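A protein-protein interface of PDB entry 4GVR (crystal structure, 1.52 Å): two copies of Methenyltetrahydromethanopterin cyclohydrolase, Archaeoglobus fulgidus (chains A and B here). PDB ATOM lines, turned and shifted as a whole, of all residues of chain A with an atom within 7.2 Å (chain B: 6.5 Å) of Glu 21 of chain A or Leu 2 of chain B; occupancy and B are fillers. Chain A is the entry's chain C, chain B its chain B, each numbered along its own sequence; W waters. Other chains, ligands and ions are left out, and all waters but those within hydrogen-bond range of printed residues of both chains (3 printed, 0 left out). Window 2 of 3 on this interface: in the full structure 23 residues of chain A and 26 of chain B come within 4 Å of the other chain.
No position is printed for both chains. Of the 8 pairs that touch across the chains among the printed residues, none has its exchanged pair printed and touching as well.
Among the printed residues, merely in contact across the chains: Glu 20 of chain A with Leu 2 of chain B (3.7 Å), Glu 20 of chain A with His 84 of chain B (3.8 Å), Glu 21 of chain A with Leu 2 of chain B (3.7 Å), Glu 21 of chain A with His 84 of chain B (2.9 Å), Arg 23 of chain A with His 84 of chain B (3.7 Å) and Ser 45 of chain A with Asp 83 of chain B (3.4 Å).
O of Arg 23 of chain A sits at hydrogen-bond distance from N of Gly 44 of chain A, at 2.8 Å. The side-chain hydroxyl (OG) of Ser 45 of chain A is in hydrogen-bond range of the backbone carbonyl oxygen (O) of Leu 22 of chain A (2.6 Å). The side-chain hydroxyl (OG) of Ser 45 of chain A sits at hydrogen-bond distance from the backbone NH (N) of Ala 48 of chain A (3.0 Å). The backbone carbonyl oxygen (O) of Leu 2 of chain B sits at hydrogen-bond distance from the side-chain hydroxyl (OH) of Tyr 128 of chain B (2.7 Å).
Of the 13 printed residues of chain A, 4 touch a printed residue of chain B. Printed residues of chain A that touch a printed residue of chain B: Glu 20, Glu 21, Arg 23 and Ser 45. Of the 14 printed residues of chain B, 4 touch a printed residue of chain A. Hydrophobic or aromatic side chains of chain B within 4 Å of the printed part of chain A: Leu 2 and His 84. Along chain B the printed residues that touch a printed residue of chain A span positions 1 to 84. Among the printed residues, 8 pairs touch across the chains.
Of chain B, only Leu 2 and His 84 come within 4 Å of Glu 21 of chain A. Of the printed residues of chain A, Met 1 of chain B touches Glu 20. Printed residues of chain B within 4 Å of Glu 20 of chain A: Met 1 (2.8 Å), Leu 2 (3.7 Å) and His 84 (3.8 Å). Of the printed residues of chain A, His 84 of chain B touches Glu 20, Glu 21 and Arg 23. Tyr 18 of chain A touches none of the printed residues of chain B. The nearest residue of chain A that does not touch Leu 2 of chain B is Leu 22 of chain A (6.5 Å).
The guanidinium group (NH2) of Arg 23 of chain A lies within salt-bridge range of the side-chain carboxylate (OD2) of Asp 83 of chain B. The backbone NH (N) of Met 1 of chain B lies within hydrogen-bond range of the side-chain carboxylate (OE1) of Glu 20 of chain A, at 2.8 Å.
Water W3 bridges the backbone carbonyl oxygen (O) of Glu 20 of chain A (2.7 Å) and a ring nitrogen (NE2) of His 84 of chain B (2.9 Å). Water W1 lies within hydrogen-bond range of the side-chain carboxylate of Asp 83 of chain B (2.8 Å) and the backbone NH of Asp 47 of chain A (3.0 Å). Water W2 bridges O of Asp 83 of chain B (3.0 Å) and NH1 of Arg 23 of chain A (3.2 Å).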
ATOM      1  N   MET A  15     -23.541   5.852   0.318  1.00  0.00           N
ATOM      2  CA  MET A  15     -23.367   4.544   1.020  1.00  0.00           C
ATOM      3  C   MET A  15     -21.905   4.306   1.399  1.00  0.00           C
ATOM      4  O   MET A  15     -21.594   3.896   2.511  1.00  0.00           O
ATOM      5  CB  MET A  15     -23.866   3.362   0.202  1.00  0.00           C
ATOM      6  CG  MET A  15     -25.339   3.425  -0.142  1.00  0.00           C
ATOM      7  SD  MET A  15     -25.888   2.117  -1.270  1.00  0.00           S
ATOM      8  CE  MET A  15     -26.133   0.795  -0.029  1.00  0.00           C
ATOM      9  N   ASP A  17     -19.687   6.335   2.134  1.00  0.00           N
ATOM     10  CA  ASP A  17     -19.287   7.254   3.206  1.00  0.00           C
ATOM     11  C   ASP A  17     -19.706   6.805   4.617  1.00  0.00           C
ATOM     12  O   ASP A  17     -19.206   7.334   5.582  1.00  0.00           O
ATOM     13  CB  ASP A  17     -19.814   8.676   2.897  1.00  0.00           C
ATOM     14  CG  ASP A  17     -18.999   9.368   1.811  1.00  0.00           C
ATOM     15  OD1 ASP A  17     -17.881   8.926   1.517  1.00  0.00           O
ATOM     16  OD2 ASP A  17     -19.492  10.360   1.283  1.00  0.00           O
ATOM     17  N   TYR A  18     -20.641   5.852   4.703  1.00  0.00           N
ATOM     18  CA  TYR A  18     -21.225   5.398   5.975  1.00  0.00           C
ATOM     19  C   TYR A  18     -21.231   3.888   6.102  1.00  0.00           C
ATOM     20  O   TYR A  18     -22.230   3.321   6.597  1.00  0.00           O
ATOM     21  CB  TYR A  18     -22.672   5.939   6.100  1.00  0.00           C
ATOM     22  CG  TYR A  18     -22.698   7.419   6.228  1.00  0.00           C
ATOM     23  CD1 TYR A  18     -22.527   8.011   7.482  1.00  0.00           C
ATOM     24  CD2 TYR A  18     -22.808   8.252   5.096  1.00  0.00           C
ATOM     25  CE1 TYR A  18     -22.495   9.381   7.636  1.00  0.00           C
ATOM     26  CE2 TYR A  18     -22.779   9.629   5.241  1.00  0.00           C
ATOM     27  CZ  TYR A  18     -22.619  10.193   6.518  1.00  0.00           C
ATOM     28  OH  TYR A  18     -22.574  11.573   6.688  1.00  0.00           O
ATOM     29  N   GLU A  19     -20.174   3.223   5.605  1.00  0.00           N
ATOM     30  CA  GLU A  19     -20.230   1.743   5.585  1.00  0.00           C
ATOM     31  C   GLU A  19     -20.407   1.062   6.954  1.00  0.00           C
ATOM     32  O   GLU A  19     -21.218   0.136   7.071  1.00  0.00           O
ATOM     33  CB  GLU A  19     -19.071   1.090   4.849  1.00  0.00           C
ATOM     34  CG  GLU A  19     -18.687   1.764   3.513  1.00  0.00           C
ATOM     35  CD  GLU A  19     -17.842   0.891   2.605  1.00  0.00           C
ATOM     36  OE1 GLU A  19     -17.446  -0.221   3.010  1.00  0.00           O
ATOM     37  OE2 GLU A  19     -17.551   1.351   1.470  1.00  0.00           O
ATOM     38  N   GLU A  20     -19.672   1.514   7.968  1.00  0.00           N
ATOM     39  CA  GLU A  20     -19.736   0.855   9.253  1.00  0.00           C
ATOM     40  C   GLU A  20     -21.136   1.056   9.826  1.00  0.00           C
ATOM     41  O   GLU A  20     -21.715   0.122  10.366  1.00  0.00           O
ATOM     42  CB  GLU A  20     -18.677   1.358  10.217  1.00  0.00           C
ATOM     43  CG  GLU A  20     -18.631   0.538  11.506  1.00  0.00           C
ATOM     44  CD  GLU A  20     -17.381   0.783  12.327  1.00  0.00           C
ATOM     45  OE1 GLU A  20     -16.500   1.591  11.957  1.00  0.00           O
ATOM     46  OE2 GLU A  20     -17.279   0.149  13.389  1.00  0.00           O
ATOM     47  N   GLU A  21     -21.669   2.278   9.697  1.00  0.00           N
ATOM     48  CA  GLU A  21     -23.010   2.596  10.198  1.00  0.00           C
ATOM     49  C   GLU A  21     -24.076   1.714   9.518  1.00  0.00           C
ATOM     50  O   GLU A  21     -24.958   1.154  10.169  1.00  0.00           O
ATOM     51  CB  GLU A  21     -23.330   4.076   9.957  1.00  0.00           C
ATOM     52  CG  GLU A  21     -22.464   5.031  10.768  1.00  0.00           C
ATOM     53  CD  GLU A  21     -21.120   5.485  10.105  1.00  0.00           C
ATOM     54  OE1 GLU A  21     -20.488   4.752   9.241  1.00  0.00           O
ATOM     55  OE2 GLU A  21     -20.680   6.621  10.484  1.00  0.00           O
ATOM     56  N   LEU A  22     -23.971   1.563   8.201  1.00  0.00           N
ATOM     57  CA  LEU A  22     -24.926   0.803   7.396  1.00  0.00           C
ATOM     58  C   LEU A  22     -24.664  -0.711   7.448  1.00  0.00           C
ATOM     59  O   LEU A  22     -25.506  -1.493   6.937  1.00  0.00           O
ATOM     60  CB  LEU A  22     -24.843   1.279   5.937  1.00  0.00           C
ATOM     61  CG  LEU A  22     -25.300   2.749   5.629  1.00  0.00           C
ATOM     62  CD1 LEU A  22     -24.842   3.131   4.184  1.00  0.00           C
ATOM     63  CD2 LEU A  22     -26.844   2.826   5.896  1.00  0.00           C
ATOM     64  N   ARG A  23     -23.514  -1.101   8.023  1.00  0.00           N
ATOM     65  CA  ARG A  23     -23.068  -2.495   8.142  1.00  0.00           C
ATOM     66  C   ARG A  23     -22.921  -3.150   6.762  1.00  0.00           C
ATOM     67  O   ARG A  23     -23.405  -4.263   6.521  1.00  0.00           O
ATOM     68  CB  ARG A  23     -24.002  -3.333   9.065  1.00  0.00           C
ATOM     69  CG  ARG A  23     -24.330  -2.739  10.451  1.00  0.00           C
ATOM     70  CD  ARG A  23     -24.896  -3.780  11.455  1.00  0.00           C
ATOM     71  NE  ARG A  23     -26.256  -4.183  11.097  1.00  0.00           N
ATOM     72  CZ  ARG A  23     -27.015  -5.107  11.720  1.00  0.00           C
ATOM     73  NH1 ARG A  23     -26.560  -5.794  12.761  1.00  0.00           N
ATOM     74  NH2 ARG A  23     -28.249  -5.361  11.270  1.00  0.00           N
ATOM     75  N   ILE A  24     -22.242  -2.431   5.857  1.00  0.00           N
ATOM     76  CA  ILE A  24     -21.929  -2.916   4.527  1.00  0.00           C
ATOM     77  C   ILE A  24     -20.400  -2.877   4.390  1.00  0.00           C
ATOM     78  O   ILE A  24     -19.687  -2.324   5.245  1.00  0.00           O
ATOM     79  CB  ILE A  24     -22.661  -2.109   3.407  1.00  0.00           C
ATOM     80  CG1 ILE A  24     -22.123  -0.636   3.327  1.00  0.00           C
ATOM     81  CG2 ILE A  24     -24.206  -2.301   3.664  1.00  0.00           C
ATOM     82  CD1 ILE A  24     -22.864   0.290   2.409  1.00  0.00           C
ATOM     83  N   GLY A  44     -25.682  -5.941   6.636  1.00  0.00           N
ATOM     84  CA  GLY A  44     -26.507  -4.874   6.088  1.00  0.00           C
ATOM     85  C   GLY A  44     -27.442  -4.285   7.171  1.00  0.00           C
ATOM     86  O   GLY A  44     -27.253  -4.528   8.402  1.00  0.00           O
ATOM     87  N   SER A  45     -28.461  -3.527   6.740  1.00  0.00           N
ATOM     88  CA  SER A  45     -29.244  -2.755   7.716  1.00  0.00           C
ATOM     89  C   SER A  45     -30.509  -2.260   7.040  1.00  0.00           C
ATOM     90  O   SER A  45     -30.624  -2.307   5.804  1.00  0.00           O
ATOM     91  CB  SER A  45     -28.486  -1.516   8.254  1.00  0.00           C
ATOM     92  OG  SER A  45     -28.022  -0.709   7.122  1.00  0.00           O
ATOM     93  N   ASP A  47     -31.472   0.866   6.792  1.00  0.00           N
ATOM     94  CA  ASP A  47     -31.025   1.982   5.892  1.00  0.00           C
ATOM     95  C   ASP A  47     -30.259   1.529   4.626  1.00  0.00           C
ATOM     96  O   ASP A  47     -30.485   2.126   3.540  1.00  0.00           O
ATOM     97  CB  ASP A  47     -30.263   3.021   6.681  1.00  0.00           C
ATOM     98  CG  ASP A  47     -31.204   3.909   7.518  1.00  0.00           C
ATOM     99  OD1 ASP A  47     -32.459   3.960   7.218  1.00  0.00           O
ATOM    100  OD2 ASP A  47     -30.665   4.561   8.461  1.00  0.00           O
ATOM    101  N   ALA A  48     -29.417   0.493   4.727  1.00  0.00           N
ATOM    102  CA  ALA A  48     -28.749   0.003   3.498  1.00  0.00           C
ATOM    103  C   ALA A  48     -29.838  -0.525   2.574  1.00  0.00           C
ATOM    104  O   ALA A  48     -29.753  -0.372   1.342  1.00  0.00           O
ATOM    105  CB  ALA A  48     -27.714  -1.072   3.769  1.00  0.00           C
ATOM    106  N   MET B   1     -14.558   2.028  13.917  1.00  0.00           N
ATOM    107  CA  MET B   1     -15.319   2.071  15.207  1.00  0.00           C
ATOM    108  C   MET B   1     -16.424   3.142  15.143  1.00  0.00           C
ATOM    109  O   MET B   1     -16.275   4.144  14.468  1.00  0.00           O
ATOM    110  CB  MET B   1     -14.298   2.317  16.335  1.00  0.00           C
ATOM    111  CG  MET B   1     -14.836   2.324  17.746  1.00  0.00           C
ATOM    112  SD  MET B   1     -15.026   4.024  18.324  1.00  0.00           S
ATOM    113  CE  MET B   1     -15.601   3.753  19.990  1.00  0.00           C
ATOM    114  N   LEU B   2     -17.574   2.904  15.815  1.00  0.00           N
ATOM    115  CA  LEU B   2     -18.644   3.910  15.846  1.00  0.00           C
ATOM    116  C   LEU B   2     -18.594   4.617  17.171  1.00  0.00           C
ATOM    117  O   LEU B   2     -18.699   3.961  18.207  1.00  0.00           O
ATOM    118  CB  LEU B   2     -20.030   3.225  15.685  1.00  0.00           C
ATOM    119  CG  LEU B   2     -20.241   2.536  14.327  1.00  0.00           C
ATOM    120  CD1 LEU B   2     -21.587   1.852  14.219  1.00  0.00           C
ATOM    121  CD2 LEU B   2     -20.072   3.559  13.222  1.00  0.00           C
ATOM    122  N   SER B   3     -18.428   5.940  17.141  1.00  0.00           N
ATOM    123  CA  SER B   3     -18.336   6.741  18.349  1.00  0.00           C
ATOM    124  C   SER B   3     -19.662   7.443  18.613  1.00  0.00           C
ATOM    125  O   SER B   3     -19.971   8.455  17.919  1.00  0.00           O
ATOM    126  CB  SER B   3     -17.231   7.799  18.214  1.00  0.00           C
ATOM    127  OG  SER B   3     -17.268   8.699  19.310  1.00  0.00           O
ATOM    128  N   VAL B   4     -20.481   6.900  19.556  1.00  0.00           N
ATOM    129  CA  VAL B   4     -21.764   7.524  19.886  1.00  0.00           C
ATOM    130  C   VAL B   4     -21.628   9.007  20.281  1.00  0.00           C
ATOM    131  O   VAL B   4     -22.499   9.820  19.933  1.00  0.00           O
ATOM    132  CB  VAL B   4     -22.606   6.749  20.917  1.00  0.00           C
ATOM    133  CG1 VAL B   4     -23.169   5.447  20.312  1.00  0.00           C
ATOM    134  CG2 VAL B   4     -21.904   6.545  22.259  1.00  0.00           C
ATOM    135  N   ASN B   5     -20.501   9.375  20.925  1.00  0.00           N
ATOM    136  CA  ASN B   5     -20.353  10.783  21.311  1.00  0.00           C
ATOM    137  C   ASN B   5     -20.102  11.674  20.109  1.00  0.00           C
ATOM    138  O   ASN B   5     -20.702  12.762  19.981  1.00  0.00           O
ATOM    139  CB  ASN B   5     -19.334  10.983  22.432  1.00  0.00           C
ATOM    140  CG  ASN B   5     -19.844  10.440  23.756  1.00  0.00           C
ATOM    141  OD1 ASN B   5     -19.584   9.261  24.122  1.00  0.00           O
ATOM    142  ND2 ASN B   5     -20.611  11.256  24.464  1.00  0.00           N
ATOM    143  N   ILE B   7     -20.705  11.103  16.921  1.00  0.00           N
ATOM    144  CA  ILE B   7     -21.876  11.104  16.014  1.00  0.00           C
ATOM    145  C   ILE B   7     -22.964  12.027  16.540  1.00  0.00           C
ATOM    146  O   ILE B   7     -23.519  12.838  15.789  1.00  0.00           O
ATOM    147  CB  ILE B   7     -22.348   9.676  15.681  1.00  0.00           C
ATOM    148  CG1 ILE B   7     -21.222   8.906  14.946  1.00  0.00           C
ATOM    149  CG2 ILE B   7     -23.633   9.734  14.857  1.00  0.00           C
ATOM    150  CD1 ILE B   7     -21.447   7.393  14.859  1.00  0.00           C
ATOM    151  N   GLY B  59     -26.900   8.757  17.646  1.00  0.00           N
ATOM    152  CA  GLY B  59     -27.023   8.900  16.205  1.00  0.00           C
ATOM    153  C   GLY B  59     -27.026   7.606  15.399  1.00  0.00           C
ATOM    154  O   GLY B  59     -26.810   7.634  14.177  1.00  0.00           O
ATOM    155  N   LEU B  60     -27.276   6.471  16.067  1.00  0.00           N
ATOM    156  CA  LEU B  60     -27.300   5.155  15.430  1.00  0.00           C
ATOM    157  C   LEU B  60     -28.752   4.594  15.216  1.00  0.00           C
ATOM    158  O   LEU B  60     -28.941   3.385  15.033  1.00  0.00           O
ATOM    159  CB  LEU B  60     -26.436   4.167  16.219  1.00  0.00           C
ATOM    160  CG  LEU B  60     -24.930   4.506  16.295  1.00  0.00           C
ATOM    161  CD1 LEU B  60     -24.210   3.450  17.138  1.00  0.00           C
ATOM    162  CD2 LEU B  60     -24.319   4.604  14.915  1.00  0.00           C
ATOM    163  N   ASP B  83     -30.094  -0.644  13.604  1.00  0.00           N
ATOM    164  CA  ASP B  83     -29.322  -1.863  13.396  1.00  0.00           C
ATOM    165  C   ASP B  83     -28.096  -1.959  14.329  1.00  0.00           C
ATOM    166  O   ASP B  83     -27.187  -2.783  14.102  1.00  0.00           O
ATOM    167  CB  ASP B  83     -28.926  -1.956  11.921  1.00  0.00           C
ATOM    168  CG  ASP B  83     -30.111  -2.382  11.074  1.00  0.00           C
ATOM    169  OD1 ASP B  83     -30.887  -1.482  10.660  1.00  0.00           O
ATOM    170  OD2 ASP B  83     -30.301  -3.618  10.904  1.00  0.00           O
ATOM    171  N   HIS B  84     -28.092  -1.110  15.364  1.00  0.00           N
ATOM    172  CA  HIS B  84     -27.162  -1.180  16.473  1.00  0.00           C
ATOM    173  C   HIS B  84     -27.895  -1.121  17.816  1.00  0.00           C
ATOM    174  O   HIS B  84     -27.622  -0.265  18.626  1.00  0.00           O
ATOM    175  CB  HIS B  84     -26.158  -0.048  16.356  1.00  0.00           C
ATOM    176  CG  HIS B  84     -25.337  -0.122  15.067  1.00  0.00           C
ATOM    177  ND1 HIS B  84     -25.732   0.457  13.904  1.00  0.00           N
ATOM    178  CD2 HIS B  84     -24.154  -0.796  14.794  1.00  0.00           C
ATOM    179  CE1 HIS B  84     -24.824   0.205  12.937  1.00  0.00           C
ATOM    180  NE2 HIS B  84     -23.859  -0.581  13.478  1.00  0.00           N
ATOM    181  N   ILE B  87     -25.718  -1.103  21.346  1.00  0.00           N
ATOM    182  CA  ILE B  87     -24.954   0.162  21.507  1.00  0.00           C
ATOM    183  C   ILE B  87     -25.937   1.355  21.638  1.00  0.00           C
ATOM    184  O   ILE B  87     -25.869   2.154  22.592  1.00  0.00           O
ATOM    185  CB  ILE B  87     -23.921   0.451  20.361  1.00  0.00           C
ATOM    186  CG1 ILE B  87     -22.765  -0.619  20.312  1.00  0.00           C
ATOM    187  CG2 ILE B  87     -23.315   1.850  20.518  1.00  0.00           C
ATOM    188  CD1 ILE B  87     -21.852  -0.560  19.069  1.00  0.00           C
ATOM    189  N   TYR B 128     -18.834  -2.750  24.555  1.00  0.00           N
ATOM    190  CA  TYR B 128     -18.652  -1.465  23.904  1.00  0.00           C
ATOM    191  C   TYR B 128     -18.076  -0.450  24.896  1.00  0.00           C
ATOM    192  O   TYR B 128     -18.458  -0.427  26.085  1.00  0.00           O
ATOM    193  CB  TYR B 128     -19.971  -0.924  23.369  1.00  0.00           C
ATOM    194  CG  TYR B 128     -19.842   0.420  22.688  1.00  0.00           C
ATOM    195  CD1 TYR B 128     -19.355   0.513  21.384  1.00  0.00           C
ATOM    196  CD2 TYR B 128     -20.217   1.611  23.331  1.00  0.00           C
ATOM    197  CE1 TYR B 128     -19.215   1.741  20.737  1.00  0.00           C
ATOM    198  CE2 TYR B 128     -20.074   2.849  22.703  1.00  0.00           C
ATOM    199  CZ  TYR B 128     -19.574   2.918  21.393  1.00  0.00           C
ATOM    200  OH  TYR B 128     -19.434   4.147  20.748  1.00  0.00           O
ATOM    201  N   GLU B 129     -17.166   0.374  24.402  1.00  0.00           N
ATOM    202  CA  GLU B 129     -16.688   1.571  25.120  1.00  0.00           C
ATOM    203  C   GLU B 129     -16.352   2.612  24.056  1.00  0.00           C
ATOM    204  O   GLU B 129     -15.767   2.292  23.016  1.00  0.00           O
ATOM    205  CB  GLU B 129     -15.441   1.266  25.963  1.00  0.00           C
ATOM    206  CG  GLU B 129     -15.027   2.408  26.883  1.00  0.00           C
ATOM    207  CD  GLU B 129     -13.785   2.099  27.716  1.00  0.00           C
ATOM    208  OE1 GLU B 129     -13.337   0.917  27.733  1.00  0.00           O
ATOM    209  OE2 GLU B 129     -13.271   3.048  28.377  1.00  0.00           O
ATOM    210  N   ASP B 130     -16.737   3.854  24.307  1.00  0.00           N
ATOM    211  CA  ASP B 130     -16.441   4.922  23.379  1.00  0.00           C
ATOM    212  C   ASP B 130     -15.079   5.523  23.740  1.00  0.00           C
ATOM    213  O   ASP B 130     -14.665   5.454  24.877  1.00  0.00           O
ATOM    214  CB  ASP B 130     -17.538   5.980  23.421  1.00  0.00           C
ATOM    215  CG  ASP B 130     -17.536   6.900  22.183  1.00  0.00           C
ATOM    216  OD1 ASP B 130     -16.648   6.784  21.289  1.00  0.00           O
ATOM    217  OD2 ASP B 130     -18.441   7.749  22.099  1.00  0.00           O
HETATM  218  O   HOH W   1     -30.595   1.147   9.615  1.00  0.00           O
HETATM  219  O   HOH W   2     -26.726  -5.204  15.868  1.00  0.00           O
HETATM  220  O   HOH W   3     -21.391  -1.672  12.385  1.00  0.00           O
